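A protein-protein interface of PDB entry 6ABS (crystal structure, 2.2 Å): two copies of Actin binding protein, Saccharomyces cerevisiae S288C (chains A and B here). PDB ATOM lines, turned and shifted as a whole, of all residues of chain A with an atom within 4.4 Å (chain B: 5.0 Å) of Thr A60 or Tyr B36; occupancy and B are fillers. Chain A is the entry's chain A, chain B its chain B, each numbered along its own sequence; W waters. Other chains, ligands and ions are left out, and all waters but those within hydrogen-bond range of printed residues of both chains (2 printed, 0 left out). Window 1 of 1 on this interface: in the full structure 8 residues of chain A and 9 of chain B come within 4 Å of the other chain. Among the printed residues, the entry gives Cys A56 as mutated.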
ATOM      1  N   CYS A  56      11.368  -7.754  -9.322  1.00  0.00           N
ATOM      2  CA  CYS A  56       9.998  -7.421  -8.892  1.00  0.00           C
ATOM      3  C   CYS A  56       9.670  -8.010  -7.519  1.00  0.00           C
ATOM      4  O   CYS A  56       9.139  -7.326  -6.641  1.00  0.00           O
ATOM      5  CB  CYS A  56       8.977  -7.922  -9.923  1.00  0.00           C
ATOM      6  SG  CYS A  56       7.238  -7.824  -9.398  1.00  0.00           S
ATOM      7  N   THR A  57       9.993  -9.285  -7.343  1.00  0.00           N
ATOM      8  CA  THR A  57       9.713  -9.974  -6.083  1.00  0.00           C
ATOM      9  C   THR A  57      10.522  -9.377  -4.953  1.00  0.00           C
ATOM     10  O   THR A  57      10.011  -9.172  -3.851  1.00  0.00           O
ATOM     11  CB  THR A  57      10.005 -11.492  -6.186  1.00  0.00           C
ATOM     12  OG1 THR A  57       9.101 -12.075  -7.130  1.00  0.00           O
ATOM     13  CG2 THR A  57       9.824 -12.193  -4.818  1.00  0.00           C
ATOM     14  N   ILE A  58      11.780  -9.070  -5.235  1.00  0.00           N
ATOM     15  CA  ILE A  58      12.642  -8.465  -4.236  1.00  0.00           C
ATOM     16  C   ILE A  58      12.116  -7.084  -3.802  1.00  0.00           C
ATOM     17  O   ILE A  58      11.955  -6.824  -2.607  1.00  0.00           O
ATOM     18  CB  ILE A  58      14.091  -8.361  -4.765  1.00  0.00           C
ATOM     19  CG1 ILE A  58      14.742  -9.752  -4.791  1.00  0.00           C
ATOM     20  CG2 ILE A  58      14.909  -7.394  -3.920  1.00  0.00           C
ATOM     21  CD1 ILE A  58      16.126  -9.762  -5.436  1.00  0.00           C
ATOM     22  N   LEU A  59      11.821  -6.212  -4.761  1.00  0.00           N
ATOM     23  CA  LEU A  59      11.300  -4.892  -4.431  1.00  0.00           C
ATOM     24  C   LEU A  59       9.969  -5.017  -3.701  1.00  0.00           C
ATOM     25  O   LEU A  59       9.718  -4.313  -2.720  1.00  0.00           O
ATOM     26  CB  LEU A  59      11.136  -4.031  -5.696  1.00  0.00           C
ATOM     27  CG  LEU A  59      12.297  -3.056  -5.951  1.00  0.00           C
ATOM     28  CD1 LEU A  59      13.601  -3.813  -6.064  1.00  0.00           C
ATOM     29  CD2 LEU A  59      12.067  -2.142  -7.171  1.00  0.00           C
ATOM     30  N   THR A  60       9.120  -5.919  -4.179  1.00  0.00           N
ATOM     31  CA  THR A  60       7.837  -6.133  -3.533  1.00  0.00           C
ATOM     32  C   THR A  60       8.026  -6.583  -2.087  1.00  0.00           C
ATOM     33  O   THR A  60       7.402  -6.021  -1.189  1.00  0.00           O
ATOM     34  CB  THR A  60       6.987  -7.161  -4.290  1.00  0.00           C
ATOM     35  OG1 THR A  60       6.716  -6.678  -5.619  1.00  0.00           O
ATOM     36  CG2 THR A  60       5.681  -7.409  -3.554  1.00  0.00           C
ATOM     37  N   ALA A  61       8.905  -7.560  -1.856  1.00  0.00           N
ATOM     38  CA  ALA A  61       9.166  -8.033  -0.496  1.00  0.00           C
ATOM     39  C   ALA A  61       9.785  -6.952   0.408  1.00  0.00           C
ATOM     40  O   ALA A  61       9.606  -6.979   1.625  1.00  0.00           O
ATOM     41  CB  ALA A  61      10.061  -9.251  -0.525  1.00  0.00           C
ATOM     42  N   ASN A  62      10.516  -6.006  -0.177  1.00  0.00           N
ATOM     43  CA  ASN A  62      11.059  -4.906   0.604  1.00  0.00           C
ATOM     44  C   ASN A  62      10.083  -3.740   0.728  1.00  0.00           C
ATOM     45  O   ASN A  62      10.449  -2.667   1.220  1.00  0.00           O
ATOM     46  CB  ASN A  62      12.381  -4.416  -0.005  1.00  0.00           C
ATOM     47  CG  ASN A  62      13.567  -5.282   0.401  1.00  0.00           C
ATOM     48  OD1 ASN A  62      14.295  -4.953   1.335  1.00  0.00           O
ATOM     49  ND2 ASN A  62      13.770  -6.386  -0.311  1.00  0.00           N
ATOM     50  N   ARG A  63       8.848  -3.949   0.279  1.00  0.00           N
ATOM     51  CA  ARG A  63       7.836  -2.896   0.274  1.00  0.00           C
ATOM     52  C   ARG A  63       8.322  -1.646  -0.469  1.00  0.00           C
ATOM     53  O   ARG A  63       8.090  -0.527  -0.022  1.00  0.00           O
ATOM     54  CB  ARG A  63       7.428  -2.519   1.710  1.00  0.00           C
ATOM     55  CG  ARG A  63       7.023  -3.714   2.573  1.00  0.00           C
ATOM     56  CD  ARG A  63       6.066  -4.623   1.816  1.00  0.00           C
ATOM     57  NE  ARG A  63       5.580  -5.720   2.648  1.00  0.00           N
ATOM     58  CZ  ARG A  63       5.437  -6.974   2.227  1.00  0.00           C
ATOM     59  NH1 ARG A  63       5.744  -7.296   0.978  1.00  0.00           N
ATOM     60  NH2 ARG A  63       4.990  -7.904   3.058  1.00  0.00           N
ATOM     61  N   PHE A  66       7.210   0.416  -7.211  1.00  0.00           N
ATOM     62  CA  PHE A  66       7.955   0.594  -8.452  1.00  0.00           C
ATOM     63  C   PHE A  66       7.053   0.408  -9.656  1.00  0.00           C
ATOM     64  O   PHE A  66       5.949  -0.131  -9.543  1.00  0.00           O
ATOM     65  CB  PHE A  66       9.094  -0.412  -8.547  1.00  0.00           C
ATOM     66  CG  PHE A  66       8.614  -1.823  -8.736  1.00  0.00           C
ATOM     67  CD1 PHE A  66       8.259  -2.592  -7.647  1.00  0.00           C
ATOM     68  CD2 PHE A  66       8.484  -2.368 -10.007  1.00  0.00           C
ATOM     69  CE1 PHE A  66       7.806  -3.886  -7.811  1.00  0.00           C
ATOM     70  CE2 PHE A  66       8.013  -3.667 -10.174  1.00  0.00           C
ATOM     71  CZ  PHE A  66       7.681  -4.427  -9.071  1.00  0.00           C
ATOM     72  N   PRO B  34       3.300  -3.941 -12.016  1.00  0.00           N
ATOM     73  CA  PRO B  34       3.483  -5.388 -11.863  1.00  0.00           C
ATOM     74  C   PRO B  34       2.144  -6.091 -11.663  1.00  0.00           C
ATOM     75  O   PRO B  34       1.261  -5.538 -11.005  1.00  0.00           O
ATOM     76  CB  PRO B  34       4.357  -5.497 -10.609  1.00  0.00           C
ATOM     77  CG  PRO B  34       4.013  -4.274  -9.816  1.00  0.00           C
ATOM     78  CD  PRO B  34       3.801  -3.192 -10.845  1.00  0.00           C
ATOM     79  N   VAL B  35       1.991  -7.283 -12.234  1.00  0.00           N
ATOM     80  CA  VAL B  35       0.806  -8.098 -12.002  1.00  0.00           C
ATOM     81  C   VAL B  35       1.171  -9.302 -11.136  1.00  0.00           C
ATOM     82  O   VAL B  35       2.189  -9.956 -11.342  1.00  0.00           O
ATOM     83  CB  VAL B  35       0.161  -8.572 -13.331  1.00  0.00           C
ATOM     84  CG1 VAL B  35      -1.004  -9.530 -13.069  1.00  0.00           C
ATOM     85  CG2 VAL B  35      -0.326  -7.369 -14.152  1.00  0.00           C
ATOM     86  N   TYR B  36       0.345  -9.587 -10.150  1.00  0.00           N
ATOM     87  CA  TYR B  36       0.677 -10.618  -9.180  1.00  0.00           C
ATOM     88  C   TYR B  36      -0.355 -11.731  -9.223  1.00  0.00           C
ATOM     89  O   TYR B  36      -1.541 -11.449  -9.310  1.00  0.00           O
ATOM     90  CB  TYR B  36       0.724 -10.035  -7.762  1.00  0.00           C
ATOM     91  CG  TYR B  36       1.733  -8.933  -7.517  1.00  0.00           C
ATOM     92  CD1 TYR B  36       3.094  -9.215  -7.431  1.00  0.00           C
ATOM     93  CD2 TYR B  36       1.323  -7.613  -7.342  1.00  0.00           C
ATOM     94  CE1 TYR B  36       4.024  -8.217  -7.188  1.00  0.00           C
ATOM     95  CE2 TYR B  36       2.243  -6.600  -7.088  1.00  0.00           C
ATOM     96  CZ  TYR B  36       3.597  -6.910  -7.014  1.00  0.00           C
ATOM     97  OH  TYR B  36       4.516  -5.917  -6.765  1.00  0.00           O
ATOM     98  N   ILE B  37       0.084 -12.986  -9.162  1.00  0.00           N
ATOM     99  CA  ILE B  37      -0.833 -14.055  -8.838  1.00  0.00           C
ATOM    100  C   ILE B  37      -0.808 -14.246  -7.324  1.00  0.00           C
ATOM    101  O   ILE B  37       0.210 -14.633  -6.747  1.00  0.00           O
ATOM    102  CB  ILE B  37      -0.493 -15.388  -9.585  1.00  0.00           C
ATOM    103  CG1 ILE B  37      -0.687 -15.207 -11.102  1.00  0.00           C
ATOM    104  CG2 ILE B  37      -1.384 -16.525  -9.078  1.00  0.00           C
ATOM    105  CD1 ILE B  37      -0.350 -16.450 -11.952  1.00  0.00           C
ATOM    106  N   TYR B  38      -1.921 -13.932  -6.675  1.00  0.00           N
ATOM    107  CA  TYR B  38      -2.042 -14.143  -5.237  1.00  0.00           C
ATOM    108  C   TYR B  38      -2.338 -15.609  -4.979  1.00  0.00           C
ATOM    109  O   TYR B  38      -3.306 -16.145  -5.526  1.00  0.00           O
ATOM    110  CB  TYR B  38      -3.148 -13.281  -4.642  1.00  0.00           C
ATOM    111  CG  TYR B  38      -2.744 -11.875  -4.257  1.00  0.00           C
ATOM    112  CD1 TYR B  38      -1.753 -11.188  -4.955  1.00  0.00           C
ATOM    113  CD2 TYR B  38      -3.368 -11.228  -3.188  1.00  0.00           C
ATOM    114  CE1 TYR B  38      -1.396  -9.896  -4.598  1.00  0.00           C
ATOM    115  CE2 TYR B  38      -3.025  -9.952  -2.826  1.00  0.00           C
ATOM    116  CZ  TYR B  38      -2.036  -9.283  -3.528  1.00  0.00           C
ATOM    117  OH  TYR B  38      -1.691  -7.998  -3.165  1.00  0.00           O
ATOM    118  N   PHE B  66       4.083 -11.828 -14.666  1.00  0.00           N
ATOM    119  CA  PHE B  66       3.557 -11.849 -13.316  1.00  0.00           C
ATOM    120  C   PHE B  66       4.604 -12.405 -12.370  1.00  0.00           C
ATOM    121  O   PHE B  66       5.584 -13.029 -12.801  1.00  0.00           O
ATOM    122  CB  PHE B  66       2.285 -12.706 -13.246  1.00  0.00           C
ATOM    123  CG  PHE B  66       2.529 -14.156 -13.573  1.00  0.00           C
ATOM    124  CD1 PHE B  66       2.897 -15.054 -12.584  1.00  0.00           C
ATOM    125  CD2 PHE B  66       2.438 -14.610 -14.883  1.00  0.00           C
ATOM    126  CE1 PHE B  66       3.157 -16.398 -12.888  1.00  0.00           C
ATOM    127  CE2 PHE B  66       2.675 -15.947 -15.192  1.00  0.00           C
ATOM    128  CZ  PHE B  66       3.049 -16.838 -14.186  1.00  0.00           C
ATOM    129  N   THR B  67       4.382 -12.210 -11.080  1.00  0.00           N
ATOM    130  CA  THR B  67       5.090 -12.986 -10.073  1.00  0.00           C
ATOM    131  C   THR B  67       4.084 -13.405  -9.018  1.00  0.00           C
ATOM    132  O   THR B  67       2.970 -12.878  -8.970  1.00  0.00           O
ATOM    133  CB  THR B  67       6.248 -12.206  -9.397  1.00  0.00           C
ATOM    134  OG1 THR B  67       5.734 -11.034  -8.751  1.00  0.00           O
ATOM    135  CG2 THR B  67       7.310 -11.817 -10.420  1.00  0.00           C
ATOM    136  N   TYR B  68       4.497 -14.333  -8.169  1.00  0.00           N
ATOM    137  CA  TYR B  68       3.678 -14.819  -7.067  1.00  0.00           C
ATOM    138  C   TYR B  68       3.774 -13.932  -5.859  1.00  0.00           C
ATOM    139  O   TYR B  68       4.815 -13.354  -5.584  1.00  0.00           O
ATOM    140  CB  TYR B  68       4.103 -16.218  -6.649  1.00  0.00           C
ATOM    141  CG  TYR B  68       3.864 -17.260  -7.695  1.00  0.00           C
ATOM    142  CD1 TYR B  68       2.611 -17.415  -8.271  1.00  0.00           C
ATOM    143  CD2 TYR B  68       4.892 -18.096  -8.113  1.00  0.00           C
ATOM    144  CE1 TYR B  68       2.380 -18.366  -9.250  1.00  0.00           C
ATOM    145  CE2 TYR B  68       4.677 -19.058  -9.079  1.00  0.00           C
ATOM    146  CZ  TYR B  68       3.417 -19.190  -9.644  1.00  0.00           C
ATOM    147  OH  TYR B  68       3.206 -20.153 -10.605  1.00  0.00           O
ATOM    148  N   ARG B  69       2.671 -13.828  -5.141  1.00  0.00           N
ATOM    149  CA  ARG B  69       2.726 -13.417  -3.759  1.00  0.00           C
ATOM    150  C   ARG B  69       2.025 -14.486  -2.941  1.00  0.00           C
ATOM    151  O   ARG B  69       0.873 -14.848  -3.214  1.00  0.00           O
ATOM    152  CB  ARG B  69       2.094 -12.050  -3.567  1.00  0.00           C
ATOM    153  CG  ARG B  69       2.816 -10.974  -4.361  1.00  0.00           C
ATOM    154  CD  ARG B  69       2.279  -9.604  -4.036  1.00  0.00           C
ATOM    155  NE  ARG B  69       2.704  -9.130  -2.721  1.00  0.00           N
ATOM    156  CZ  ARG B  69       2.581  -7.866  -2.351  1.00  0.00           C
ATOM    157  NH1 ARG B  69       2.077  -6.985  -3.213  1.00  0.00           N
ATOM    158  NH2 ARG B  69       2.988  -7.475  -1.153  1.00  0.00           N
ATOM    159  N   ASP B  74       3.242 -13.315   3.172  1.00  0.00           N
ATOM    160  CA  ASP B  74       3.210 -11.946   2.666  1.00  0.00           C
ATOM    161  C   ASP B  74       2.022 -11.227   3.294  1.00  0.00           C
ATOM    162  O   ASP B  74       0.868 -11.390   2.886  1.00  0.00           O
ATOM    163  CB  ASP B  74       3.136 -11.942   1.129  1.00  0.00           C
ATOM    164  CG  ASP B  74       3.232 -10.541   0.517  1.00  0.00           C
ATOM    165  OD1 ASP B  74       2.922  -9.524   1.188  1.00  0.00           O
ATOM    166  OD2 ASP B  74       3.601 -10.465  -0.676  1.00  0.00           O
ATOM    167  N   GLU B  76       1.321  -7.997   3.516  1.00  0.00           N
ATOM    168  CA  GLU B  76       0.707  -6.939   2.730  1.00  0.00           C
ATOM    169  C   GLU B  76      -0.323  -7.555   1.780  1.00  0.00           C
ATOM    170  O   GLU B  76      -1.441  -7.051   1.653  1.00  0.00           O
ATOM    171  CB  GLU B  76       1.757  -6.144   1.952  1.00  0.00           C
ATOM    172  CG  GLU B  76       1.165  -5.050   1.084  1.00  0.00           C
ATOM    173  CD  GLU B  76       2.222  -4.223   0.356  1.00  0.00           C
ATOM    174  OE1 GLU B  76       2.345  -3.019   0.645  1.00  0.00           O
ATOM    175  OE2 GLU B  76       2.926  -4.773  -0.513  1.00  0.00           O
ATOM    176  N   GLY B  92      -5.850 -15.688  -6.923  1.00  0.00           N
ATOM    177  CA  GLY B  92      -6.391 -14.570  -7.670  1.00  0.00           C
ATOM    178  C   GLY B  92      -5.287 -13.749  -8.299  1.00  0.00           C
ATOM    179  O   GLY B  92      -4.105 -14.097  -8.204  1.00  0.00           O
ATOM    180  N   VAL B  93      -5.691 -12.665  -8.955  1.00  0.00           N
ATOM    181  CA  VAL B  93      -4.782 -11.796  -9.688  1.00  0.00           C
ATOM    182  C   VAL B  93      -4.983 -10.341  -9.247  1.00  0.00           C
ATOM    183  O   VAL B  93      -6.100  -9.841  -9.252  1.00  0.00           O
ATOM    184  CB  VAL B  93      -4.998 -11.906 -11.220  1.00  0.00           C
ATOM    185  CG1 VAL B  93      -4.279 -10.787 -11.943  1.00  0.00           C
ATOM    186  CG2 VAL B  93      -4.563 -13.285 -11.758  1.00  0.00           C
ATOM    187  N   VAL B  94      -3.899  -9.683  -8.854  1.00  0.00           N
ATOM    188  CA  VAL B  94      -3.934  -8.289  -8.410  1.00  0.00           C
ATOM    189  C   VAL B  94      -2.902  -7.469  -9.186  1.00  0.00           C
ATOM    190  O   VAL B  94      -1.742  -7.859  -9.303  1.00  0.00           O
ATOM    191  CB  VAL B  94      -3.651  -8.162  -6.893  1.00  0.00           C
ATOM    192  CG1 VAL B  94      -3.645  -6.686  -6.455  1.00  0.00           C
ATOM    193  CG2 VAL B  94      -4.642  -8.990  -6.078  1.00  0.00           C
ATOM    194  N   ARG B  95      -3.337  -6.338  -9.724  1.00  0.00           N
ATOM    195  CA  ARG B  95      -2.449  -5.447 -10.446  1.00  0.00           C
ATOM    196  C   ARG B  95      -1.977  -4.324  -9.531  1.00  0.00           C
ATOM    197  O   ARG B  95      -2.777  -3.709  -8.831  1.00  0.00           O
ATOM    198  CB  ARG B  95      -3.149  -4.868 -11.674  1.00  0.00           C
ATOM    199  CG  ARG B  95      -2.247  -4.002 -12.570  1.00  0.00           C
ATOM    200  CD  ARG B  95      -3.085  -3.235 -13.603  1.00  0.00           C
ATOM    201  NE  ARG B  95      -3.988  -2.281 -12.961  1.00  0.00           N
ATOM    202  CZ  ARG B  95      -5.205  -1.984 -13.396  1.00  0.00           C
ATOM    203  NH1 ARG B  95      -5.701  -2.581 -14.472  1.00  0.00           N
ATOM    204  NH2 ARG B  95      -5.929  -1.093 -12.743  1.00  0.00           N
ATOM    205  N   GLY B  96      -0.675  -4.071  -9.543  1.00  0.00           N
ATOM    206  CA  GLY B  96      -0.084  -3.017  -8.746  1.00  0.00           C
ATOM    207  C   GLY B  96      -0.217  -3.296  -7.268  1.00  0.00           C
ATOM    208  O   GLY B  96      -0.226  -4.444  -6.822  1.00  0.00           O
HETATM  209  O   HOH W   1       4.657  -8.962 -10.497  1.00  0.00           O
HETATM  210  O   HOH W   2       6.265 -11.196  -6.222  1.00  0.00           O
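Of chain B, only Tyr B36 and Arg B69 come within 4 Å of Thr A60. Of the printed residues of chain A, Tyr B36 touches Cys A56 (3.9 Å) and Thr A60 (2.6 Å). Printed residues of chain A within 4 Å of Pro B34: Cys A56 (3.9 Å) and Phe A66 (3.7 Å). Of the printed residues of chain B, Cys A56 touches Pro B34, Tyr B36 and Thr B67. Of the printed residues of chain A, Asp B74 touches Arg A63. Printed residues of chain B within 4 Å of Phe A66: Pro B34 (3.7 Å). Ile B37 touches none of the printed residues of chain A.
Of the 16 printed residues of chain B, 6 touch a printed residue of chain A. Hydrophobic or aromatic side chains of chain B that line the printed part of chain A: Pro B34 and Tyr B36. Along chain B the printed residues that touch a printed residue of chain A span positions 34 to 76. Printed residues of chain A that touch a printed residue of chain B: Cys A56, Thr A57, Thr A60, Arg A63 and Phe A66. Hydrophobic or aromatic side chains of chain A within 4 Å of the printed part of chain B: Phe A66. Among the printed residues, Asp or Glu carboxylates within 4 Å of a Lys or Arg side-chain nitrogen of the other chain: Arg A63 with Asp B74.
Position printed for both chains: 66.
Water W2 lies within hydrogen-bond range of OG1 of Thr B67 (2.6 Å), O of Tyr B68 (2.7 Å) and OG1 of Thr A57 (3.1 Å). Water W1 lies within hydrogen-bond range of O of Val B35, OG1 of Thr B67 and SG of Cys A56.
The backbone carbonyl oxygen (O) of Cys A56 lies within hydrogen-bond range of the side-chain hydroxyl (OG1) of Thr A60, at 2.7 Å. O of Pro B34 is in hydrogen-bond range of N of Gly B96. O of Val B35 is in hydrogen-bond range of N of Thr B67, 3.2 Å away. The backbone carbonyl oxygen (O) of Thr B67 is in hydrogen-bond range of the backbone NH (N) of Ile B37. The backbone NH of Arg B69 lies within hydrogen-bond range of the backbone carbonyl oxygen of Ile B37, at 3.0 Å. The guanidinium group of Arg B69 lies within salt-bridge range of the side-chain carboxylate of Glu B76 (2.8 Å).
The side-chain hydroxyl (OG1) of Thr B67 sits at hydrogen-bond distance from the side-chain sulfur (SG) of Cys A56 (3.6 Å). The side-chain hydroxyl of Thr A60 is in hydrogen-bond range of the side-chain hydroxyl of Tyr B36. The side-chain carboxylate (OD1) of Asp B74 lies within salt-bridge range of the guanidinium group (NH2) of Arg A63 (3.2 Å). The guanidinium group (NH2) of Arg B69 lies close to the guanidinium group (NH1) of Arg A63 (3.5 Å).
Among the printed residues, pairs that only touch across the chains: Thr A60 with Arg B69 (3.4 Å), Thr A57 with Thr B67 (3.6 Å), Arg A63 with Glu B76 (3.7 Å), Phe A66 with Pro B34 (3.7 Å), Cys A56 with Pro B34 (3.9 Å) and Cys A56 with Tyr B36 (3.9 Å).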
